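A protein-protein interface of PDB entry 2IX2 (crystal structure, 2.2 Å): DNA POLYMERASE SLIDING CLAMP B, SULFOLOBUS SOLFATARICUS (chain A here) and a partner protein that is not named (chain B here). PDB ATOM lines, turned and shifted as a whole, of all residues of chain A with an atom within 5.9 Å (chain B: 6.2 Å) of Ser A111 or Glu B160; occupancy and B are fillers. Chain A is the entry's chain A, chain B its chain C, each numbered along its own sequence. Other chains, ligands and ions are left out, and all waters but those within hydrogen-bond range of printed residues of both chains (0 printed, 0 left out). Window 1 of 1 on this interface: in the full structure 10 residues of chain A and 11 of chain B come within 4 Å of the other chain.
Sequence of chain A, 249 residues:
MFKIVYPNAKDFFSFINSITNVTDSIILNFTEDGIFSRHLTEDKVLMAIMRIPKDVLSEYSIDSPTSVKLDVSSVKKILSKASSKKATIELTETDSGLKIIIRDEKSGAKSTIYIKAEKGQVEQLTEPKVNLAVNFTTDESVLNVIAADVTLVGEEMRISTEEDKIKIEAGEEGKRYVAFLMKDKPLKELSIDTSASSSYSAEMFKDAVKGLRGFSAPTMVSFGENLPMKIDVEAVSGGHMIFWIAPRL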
ATOM      1  N   LYS A  77      23.891  22.280 -12.429  1.00  0.00           N
ATOM      2  CA  LYS A  77      22.655  21.724 -11.867  1.00  0.00           C
ATOM      3  C   LYS A  77      22.063  20.528 -12.628  1.00  0.00           C
ATOM      4  O   LYS A  77      21.401  19.687 -12.029  1.00  0.00           O
ATOM      5  CB  LYS A  77      21.599  22.809 -11.593  1.00  0.00           C
ATOM      6  CG  LYS A  77      21.534  23.964 -12.587  1.00  0.00           C
ATOM      7  CD  LYS A  77      20.937  25.192 -11.903  1.00  0.00           C
ATOM      8  CE  LYS A  77      20.380  26.201 -12.917  1.00  0.00           C
ATOM      9  NZ  LYS A  77      19.572  27.277 -12.122  1.00  0.00           N
ATOM     10  N   ILE A  78      22.310  20.447 -13.932  1.00  0.00           N
ATOM     11  CA  ILE A  78      21.884  19.288 -14.718  1.00  0.00           C
ATOM     12  C   ILE A  78      22.681  18.048 -14.321  1.00  0.00           C
ATOM     13  O   ILE A  78      22.110  16.988 -14.063  1.00  0.00           O
ATOM     14  CB  ILE A  78      22.014  19.531 -16.238  1.00  0.00           C
ATOM     15  CG1 ILE A  78      21.163  20.728 -16.659  1.00  0.00           C
ATOM     16  CG2 ILE A  78      21.576  18.293 -17.020  1.00  0.00           C
ATOM     17  CD1 ILE A  78      21.734  21.490 -17.825  1.00  0.00           C
ATOM     18  N   LEU A  79      24.002  18.196 -14.262  1.00  0.00           N
ATOM     19  CA  LEU A  79      24.883  17.100 -13.861  1.00  0.00           C
ATOM     20  C   LEU A  79      24.684  16.736 -12.379  1.00  0.00           C
ATOM     21  O   LEU A  79      24.931  15.598 -11.972  1.00  0.00           O
ATOM     22  CB  LEU A  79      26.345  17.443 -14.180  1.00  0.00           C
ATOM     23  CG  LEU A  79      27.368  16.322 -14.423  1.00  0.00           C
ATOM     24  CD1 LEU A  79      26.771  15.079 -15.102  1.00  0.00           C
ATOM     25  CD2 LEU A  79      28.550  16.857 -15.228  1.00  0.00           C
ATOM     26  N   LYS A  81      21.882  16.334 -11.119  1.00  0.00           N
ATOM     27  CA  LYS A  81      20.734  15.431 -11.118  1.00  0.00           C
ATOM     28  C   LYS A  81      20.983  14.224 -12.025  1.00  0.00           C
ATOM     29  O   LYS A  81      20.239  13.242 -11.981  1.00  0.00           O
ATOM     30  CB  LYS A  81      19.461  16.169 -11.559  1.00  0.00           C
ATOM     31  CG  LYS A  81      19.145  17.465 -10.801  1.00  0.00           C
ATOM     32  CD  LYS A  81      18.678  17.215  -9.367  1.00  0.00           C
ATOM     33  CE  LYS A  81      18.220  18.517  -8.688  1.00  0.00           C
ATOM     34  NZ  LYS A  81      18.021  18.349  -7.220  1.00  0.00           N
ATOM     35  N   ALA A  82      22.037  14.302 -12.837  1.00  0.00           N
ATOM     36  CA  ALA A  82      22.316  13.286 -13.853  1.00  0.00           C
ATOM     37  C   ALA A  82      22.975  12.022 -13.303  1.00  0.00           C
ATOM     38  O   ALA A  82      22.840  10.942 -13.888  1.00  0.00           O
ATOM     39  CB  ALA A  82      23.159  13.881 -14.983  1.00  0.00           C
ATOM     40  N   ILE A 100      27.790  19.378 -24.881  1.00  0.00           N
ATOM     41  CA  ILE A 100      28.261  18.371 -23.925  1.00  0.00           C
ATOM     42  C   ILE A 100      27.396  17.111 -23.988  1.00  0.00           C
ATOM     43  O   ILE A 100      26.170  17.199 -23.967  1.00  0.00           O
ATOM     44  CB  ILE A 100      28.286  18.941 -22.486  1.00  0.00           C
ATOM     45  CG1 ILE A 100      29.429  19.955 -22.343  1.00  0.00           C
ATOM     46  CG2 ILE A 100      28.421  17.825 -21.446  1.00  0.00           C
ATOM     47  CD1 ILE A 100      29.271  20.927 -21.176  1.00  0.00           C
ATOM     48  N   ILE A 101      28.038  15.947 -24.066  1.00  0.00           N
ATOM     49  CA  ILE A 101      27.328  14.670 -24.125  1.00  0.00           C
ATOM     50  C   ILE A 101      27.677  13.780 -22.931  1.00  0.00           C
ATOM     51  O   ILE A 101      28.847  13.488 -22.678  1.00  0.00           O
ATOM     52  CB  ILE A 101      27.595  13.924 -25.460  1.00  0.00           C
ATOM     53  CG1 ILE A 101      26.895  14.638 -26.620  1.00  0.00           C
ATOM     54  CG2 ILE A 101      27.157  12.463 -25.368  1.00  0.00           C
ATOM     55  CD1 ILE A 101      27.086  13.965 -27.988  1.00  0.00           C
ATOM     56  N   ILE A 102      26.645  13.371 -22.196  1.00  0.00           N
ATOM     57  CA  ILE A 102      26.785  12.417 -21.095  1.00  0.00           C
ATOM     58  C   ILE A 102      25.945  11.196 -21.432  1.00  0.00           C
ATOM     59  O   ILE A 102      24.780  11.327 -21.815  1.00  0.00           O
ATOM     60  CB  ILE A 102      26.346  13.032 -19.741  1.00  0.00           C
ATOM     61  CG1 ILE A 102      27.133  14.312 -19.467  1.00  0.00           C
ATOM     62  CG2 ILE A 102      26.538  12.037 -18.588  1.00  0.00           C
ATOM     63  CD1 ILE A 102      26.370  15.340 -18.683  1.00  0.00           C
ATOM     64  N   ARG A 103      26.544  10.012 -21.313  1.00  0.00           N
ATOM     65  CA  ARG A 103      25.824   8.768 -21.587  1.00  0.00           C
ATOM     66  C   ARG A 103      25.867   7.755 -20.435  1.00  0.00           C
ATOM     67  O   ARG A 103      26.899   7.149 -20.146  1.00  0.00           O
ATOM     68  CB  ARG A 103      26.254   8.141 -22.929  1.00  0.00           C
ATOM     69  CG  ARG A 103      27.730   8.260 -23.271  1.00  0.00           C
ATOM     70  CD  ARG A 103      28.062   7.565 -24.600  1.00  0.00           C
ATOM     71  NE  ARG A 103      27.640   8.321 -25.788  1.00  0.00           N
ATOM     72  CZ  ARG A 103      28.380   9.238 -26.414  1.00  0.00           C
ATOM     73  NH1 ARG A 103      29.597   9.545 -25.973  1.00  0.00           N
ATOM     74  NH2 ARG A 103      27.899   9.857 -27.484  1.00  0.00           N
ATOM     75  N   ALA A 109      20.072   6.440 -21.052  1.00  0.00           N
ATOM     76  CA  ALA A 109      19.815   7.848 -21.344  1.00  0.00           C
ATOM     77  C   ALA A 109      21.041   8.562 -21.897  1.00  0.00           C
ATOM     78  O   ALA A 109      22.125   8.516 -21.304  1.00  0.00           O
ATOM     79  CB  ALA A 109      19.319   8.561 -20.092  1.00  0.00           C
ATOM     80  N   LYS A 110      20.858   9.215 -23.040  1.00  0.00           N
ATOM     81  CA  LYS A 110      21.887  10.072 -23.616  1.00  0.00           C
ATOM     82  C   LYS A 110      21.459  11.516 -23.382  1.00  0.00           C
ATOM     83  O   LYS A 110      20.447  11.962 -23.923  1.00  0.00           O
ATOM     84  CB  LYS A 110      22.060   9.778 -25.115  1.00  0.00           C
ATOM     85  CG  LYS A 110      22.999  10.730 -25.865  1.00  0.00           C
ATOM     86  CD  LYS A 110      23.176  10.283 -27.317  1.00  0.00           C
ATOM     87  CE  LYS A 110      23.508  11.450 -28.226  1.00  0.00           C
ATOM     88  NZ  LYS A 110      23.211  11.096 -29.681  1.00  0.00           N
ATOM     89  N   SER A 111      22.227  12.243 -22.573  1.00  0.00           N
ATOM     90  CA  SER A 111      21.867  13.613 -22.212  1.00  0.00           C
ATOM     91  C   SER A 111      22.854  14.636 -22.798  1.00  0.00           C
ATOM     92  O   SER A 111      24.086  14.592 -22.523  1.00  0.00           O
ATOM     93  CB  SER A 111      21.748  13.766 -20.679  1.00  0.00           C
ATOM     94  OG  SER A 111      21.157  15.023 -20.375  1.00  0.00           O
ATOM     95  N   THR A 112      22.293  15.549 -23.613  1.00  0.00           N
ATOM     96  CA  THR A 112      23.089  16.561 -24.310  1.00  0.00           C
ATOM     97  C   THR A 112      22.772  17.975 -23.828  1.00  0.00           C
ATOM     98  O   THR A 112      21.623  18.432 -23.912  1.00  0.00           O
ATOM     99  CB  THR A 112      22.892  16.500 -25.851  1.00  0.00           C
ATOM    100  OG1 THR A 112      22.833  15.134 -26.294  1.00  0.00           O
ATOM    101  CG2 THR A 112      24.030  17.210 -26.562  1.00  0.00           C
ATOM    102  N   ILE A 113      23.812  18.664 -23.346  1.00  0.00           N
ATOM    103  CA  ILE A 113      23.700  20.033 -22.855  1.00  0.00           C
ATOM    104  C   ILE A 113      24.376  21.010 -23.817  1.00  0.00           C
ATOM    105  O   ILE A 113      25.587  20.924 -24.058  1.00  0.00           O
ATOM    106  CB  ILE A 113      24.377  20.175 -21.481  1.00  0.00           C
ATOM    107  CG1 ILE A 113      24.048  18.972 -20.591  1.00  0.00           C
ATOM    108  CG2 ILE A 113      23.963  21.485 -20.819  1.00  0.00           C
ATOM    109  CD1 ILE A 113      25.126  18.653 -19.577  1.00  0.00           C
ATOM    110  N   GLY B 153      15.577   6.275 -15.418  1.00  0.00           N
ATOM    111  CA  GLY B 153      15.960   7.096 -16.555  1.00  0.00           C
ATOM    112  C   GLY B 153      14.991   8.243 -16.701  1.00  0.00           C
ATOM    113  O   GLY B 153      15.405   9.388 -16.862  1.00  0.00           O
ATOM    114  N   LYS B 155      12.831   9.504 -14.351  1.00  0.00           N
ATOM    115  CA  LYS B 155      13.086  10.370 -13.185  1.00  0.00           C
ATOM    116  C   LYS B 155      14.315  11.257 -13.373  1.00  0.00           C
ATOM    117  O   LYS B 155      14.226  12.468 -13.181  1.00  0.00           O
ATOM    118  CB  LYS B 155      13.222   9.543 -11.900  1.00  0.00           C
ATOM    119  CG  LYS B 155      13.940  10.266 -10.752  1.00  0.00           C
ATOM    120  CD  LYS B 155      13.024  10.656  -9.612  1.00  0.00           C
ATOM    121  CE  LYS B 155      13.864  11.119  -8.417  1.00  0.00           C
ATOM    122  NZ  LYS B 155      13.080  11.344  -7.153  1.00  0.00           N
ATOM    123  N   SER B 156      15.444  10.668 -13.772  1.00  0.00           N
ATOM    124  CA  SER B 156      16.671  11.444 -14.019  1.00  0.00           C
ATOM    125  C   SER B 156      16.475  12.511 -15.095  1.00  0.00           C
ATOM    126  O   SER B 156      16.905  13.651 -14.921  1.00  0.00           O
ATOM    127  CB  SER B 156      17.845  10.536 -14.404  1.00  0.00           C
ATOM    128  OG  SER B 156      18.332   9.798 -13.294  1.00  0.00           O
ATOM    129  N   ALA B 157      15.830  12.139 -16.200  1.00  0.00           N
ATOM    130  CA  ALA B 157      15.581  13.066 -17.304  1.00  0.00           C
ATOM    131  C   ALA B 157      14.674  14.226 -16.904  1.00  0.00           C
ATOM    132  O   ALA B 157      14.888  15.360 -17.328  1.00  0.00           O
ATOM    133  CB  ALA B 157      15.010  12.328 -18.535  1.00  0.00           C
ATOM    134  N   ILE B 158      13.664  13.940 -16.092  1.00  0.00           N
ATOM    135  CA  ILE B 158      12.746  14.980 -15.626  1.00  0.00           C
ATOM    136  C   ILE B 158      13.488  15.948 -14.698  1.00  0.00           C
ATOM    137  O   ILE B 158      13.433  17.155 -14.889  1.00  0.00           O
ATOM    138  CB  ILE B 158      11.449  14.376 -14.993  1.00  0.00           C
ATOM    139  CG1 ILE B 158      10.583  13.746 -16.089  1.00  0.00           C
ATOM    140  CG2 ILE B 158      10.648  15.432 -14.212  1.00  0.00           C
ATOM    141  CD1 ILE B 158      10.025  14.745 -17.097  1.00  0.00           C
ATOM    142  N   SER B 159      14.222  15.403 -13.736  1.00  0.00           N
ATOM    143  CA  SER B 159      15.036  16.208 -12.826  1.00  0.00           C
ATOM    144  C   SER B 159      16.079  17.073 -13.555  1.00  0.00           C
ATOM    145  O   SER B 159      16.194  18.269 -13.282  1.00  0.00           O
ATOM    146  CB  SER B 159      15.698  15.305 -11.788  1.00  0.00           C
ATOM    147  OG  SER B 159      14.721  14.490 -11.153  1.00  0.00           O
ATOM    148  N   GLU B 160      16.822  16.480 -14.493  1.00  0.00           N
ATOM    149  CA  GLU B 160      17.814  17.219 -15.266  1.00  0.00           C
ATOM    150  C   GLU B 160      17.176  18.409 -15.966  1.00  0.00           C
ATOM    151  O   GLU B 160      17.646  19.539 -15.836  1.00  0.00           O
ATOM    152  CB  GLU B 160      18.485  16.324 -16.313  1.00  0.00           C
ATOM    153  CG  GLU B 160      19.431  15.284 -15.757  1.00  0.00           C
ATOM    154  CD  GLU B 160      20.035  14.421 -16.850  1.00  0.00           C
ATOM    155  OE1 GLU B 160      19.963  13.168 -16.737  1.00  0.00           O
ATOM    156  OE2 GLU B 160      20.583  14.999 -17.825  1.00  0.00           O
ATOM    157  N   VAL B 161      16.102  18.142 -16.705  1.00  0.00           N
ATOM    158  CA  VAL B 161      15.442  19.160 -17.518  1.00  0.00           C
ATOM    159  C   VAL B 161      14.724  20.228 -16.669  1.00  0.00           C
ATOM    160  O   VAL B 161      14.617  21.379 -17.086  1.00  0.00           O
ATOM    161  CB  VAL B 161      14.506  18.493 -18.577  1.00  0.00           C
ATOM    162  CG1 VAL B 161      13.398  19.422 -19.025  1.00  0.00           C
ATOM    163  CG2 VAL B 161      15.327  18.010 -19.782  1.00  0.00           C
ATOM    164  N   SER B 162      14.283  19.841 -15.471  1.00  0.00           N
ATOM    165  CA  SER B 162      13.500  20.711 -14.567  1.00  0.00           C
ATOM    166  C   SER B 162      14.298  21.777 -13.815  1.00  0.00           C
ATOM    167  O   SER B 162      13.719  22.751 -13.326  1.00  0.00           O
ATOM    168  CB  SER B 162      12.726  19.859 -13.562  1.00  0.00           C
ATOM    169  OG  SER B 162      11.884  18.969 -14.262  1.00  0.00           O
ATOM    170  N   THR B 163      15.614  21.586 -13.718  1.00  0.00           N
ATOM    171  CA  THR B 163      16.506  22.572 -13.102  1.00  0.00           C
ATOM    172  C   THR B 163      16.649  23.804 -13.997  1.00  0.00           C
ATOM    173  O   THR B 163      17.163  24.837 -13.573  1.00  0.00           O
ATOM    174  CB  THR B 163      17.919  21.996 -12.842  1.00  0.00           C
ATOM    175  OG1 THR B 163      18.632  21.864 -14.080  1.00  0.00           O
ATOM    176  CG2 THR B 163      17.843  20.650 -12.166  1.00  0.00           C
ATOM    177  N   VAL B 164      16.185  23.679 -15.237  1.00  0.00           N
ATOM    178  CA  VAL B 164      16.407  24.701 -16.250  1.00  0.00           C
ATOM    179  C   VAL B 164      15.102  25.289 -16.809  1.00  0.00           C
ATOM    180  O   VAL B 164      15.100  26.384 -17.380  1.00  0.00           O
ATOM    181  CB  VAL B 164      17.357  24.150 -17.354  1.00  0.00           C
ATOM    182  CG1 VAL B 164      16.992  24.665 -18.742  1.00  0.00           C
ATOM    183  CG2 VAL B 164      18.821  24.463 -17.000  1.00  0.00           C
ATOM    184  N   VAL B 187      19.006  21.555 -23.593  1.00  0.00           N
ATOM    185  CA  VAL B 187      19.143  20.268 -22.914  1.00  0.00           C
ATOM    186  C   VAL B 187      18.213  19.251 -23.545  1.00  0.00           C
ATOM    187  O   VAL B 187      17.048  19.537 -23.776  1.00  0.00           O
ATOM    188  CB  VAL B 187      18.841  20.357 -21.394  1.00  0.00           C
ATOM    189  CG1 VAL B 187      19.120  19.027 -20.721  1.00  0.00           C
ATOM    190  CG2 VAL B 187      19.663  21.457 -20.742  1.00  0.00           C
ATOM    191  N   GLU B 188      18.733  18.059 -23.804  1.00  0.00           N
ATOM    192  CA  GLU B 188      17.993  17.005 -24.485  1.00  0.00           C
ATOM    193  C   GLU B 188      18.430  15.664 -23.928  1.00  0.00           C
ATOM    194  O   GLU B 188      19.641  15.397 -23.826  1.00  0.00           O
ATOM    195  CB  GLU B 188      18.265  17.065 -25.998  1.00  0.00           C
ATOM    196  CG  GLU B 188      17.932  15.771 -26.766  1.00  0.00           C
ATOM    197  CD  GLU B 188      18.215  15.917 -28.272  1.00  0.00           C
ATOM    198  OE1 GLU B 188      19.110  15.168 -28.799  1.00  0.00           O
ATOM    199  OE2 GLU B 188      17.549  16.785 -28.928  1.00  0.00           O
ATOM    200  N   VAL B 189      17.441  14.818 -23.563  1.00  0.00           N
ATOM    201  CA  VAL B 189      17.757  13.483 -23.085  1.00  0.00           C
ATOM    202  C   VAL B 189      17.035  12.485 -23.967  1.00  0.00           C
ATOM    203  O   VAL B 189      15.783  12.461 -23.986  1.00  0.00           O
ATOM    204  CB  VAL B 189      17.406  13.292 -21.601  1.00  0.00           C
ATOM    205  CG1 VAL B 189      17.973  11.978 -21.090  1.00  0.00           C
ATOM    206  CG2 VAL B 189      17.946  14.443 -20.784  1.00  0.00           C
ATOM    207  N   GLU B 190      17.852  11.695 -24.718  1.00  0.00           N
ATOM    208  CA  GLU B 190      17.383  10.818 -25.789  1.00  0.00           C
ATOM    209  C   GLU B 190      17.424   9.362 -25.341  1.00  0.00           C
ATOM    210  O   GLU B 190      18.460   8.799 -24.847  1.00  0.00           O
ATOM    211  CB  GLU B 190      18.247  11.012 -27.033  1.00  0.00           C
ATOM    212  CG  GLU B 190      18.030   9.989 -28.176  1.00  0.00           C
ATOM    213  CD  GLU B 190      18.931  10.215 -29.358  1.00  0.00           C
ATOM    214  OE1 GLU B 190      19.636   9.270 -29.697  1.00  0.00           O
ATOM    215  OE2 GLU B 190      18.861  11.332 -29.930  1.00  0.00           O
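Among the printed residues, merely in contact across the chains: Lys A110 with Val B189 (3.2 Å), Thr A112 with Val B187 (3.2 Å), Ser A111 with Glu B188 (3.3 Å), Ser A111 with Val B189 (3.3 Å), Lys A110 with Glu B188 (3.5 Å), Ile A78 with Glu B160 (3.5 Å), Lys A77 with Thr B163 (3.6 Å), Ile A78 with Val B187 (3.6 Å), Ala A82 with Glu B160 (3.7 Å), Lys A81 with Thr B163 (3.7 Å), Ile A78 with Thr B163 (3.8 Å), Ala A109 with Val B189 (3.8 Å), Lys A81 with Ser B159 (3.9 Å), Ala A109 with Glu B190 (3.9 Å) and Lys A81 with Glu B160 (3.96 Å).
Of the 14 printed residues of chain A, 8 touch a printed residue of chain B.
Hydrophobic or aromatic side chains of chain A within 4 Å of the printed part of chain B: Ile A78, Ala A82 and Ala A109.
The backbone NH of Thr A112 is in hydrogen-bond range of the backbone carbonyl oxygen of Glu B188.
The side-chain hydroxyl (OG) of Ser A111 is in hydrogen-bond range of the side-chain carboxylate (OE2) of Glu B160, at 2.6 Å.
The backbone NH (N) of Glu B190 lies within hydrogen-bond range of the backbone carbonyl oxygen (O) of Lys A110 (2.7 Å).
The backbone carbonyl oxygen (O) of Lys B155 is in hydrogen-bond range of the side-chain hydroxyl (OG) of Ser B159 (2.9 Å).
The backbone carbonyl oxygen of Ile A102 sits at hydrogen-bond distance from the backbone NH of Ser A111.
O of Glu B160 sits at hydrogen-bond distance from OG1 of Thr B163.
Ile A102 touches none of the printed residues of chain B.
Of the printed residues of chain B, Ala A109 touches Val B189 (3.8 Å) and Glu B190 (3.9 Å).
Ser A111 touches three residues of chain B.
Of the printed residues of chain A, Thr B163 touches Lys A77, Ile A78 and Lys A81.
The nearest residue of chain A that does not touch Glu B160 is Lys A77 (5.3 Å).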
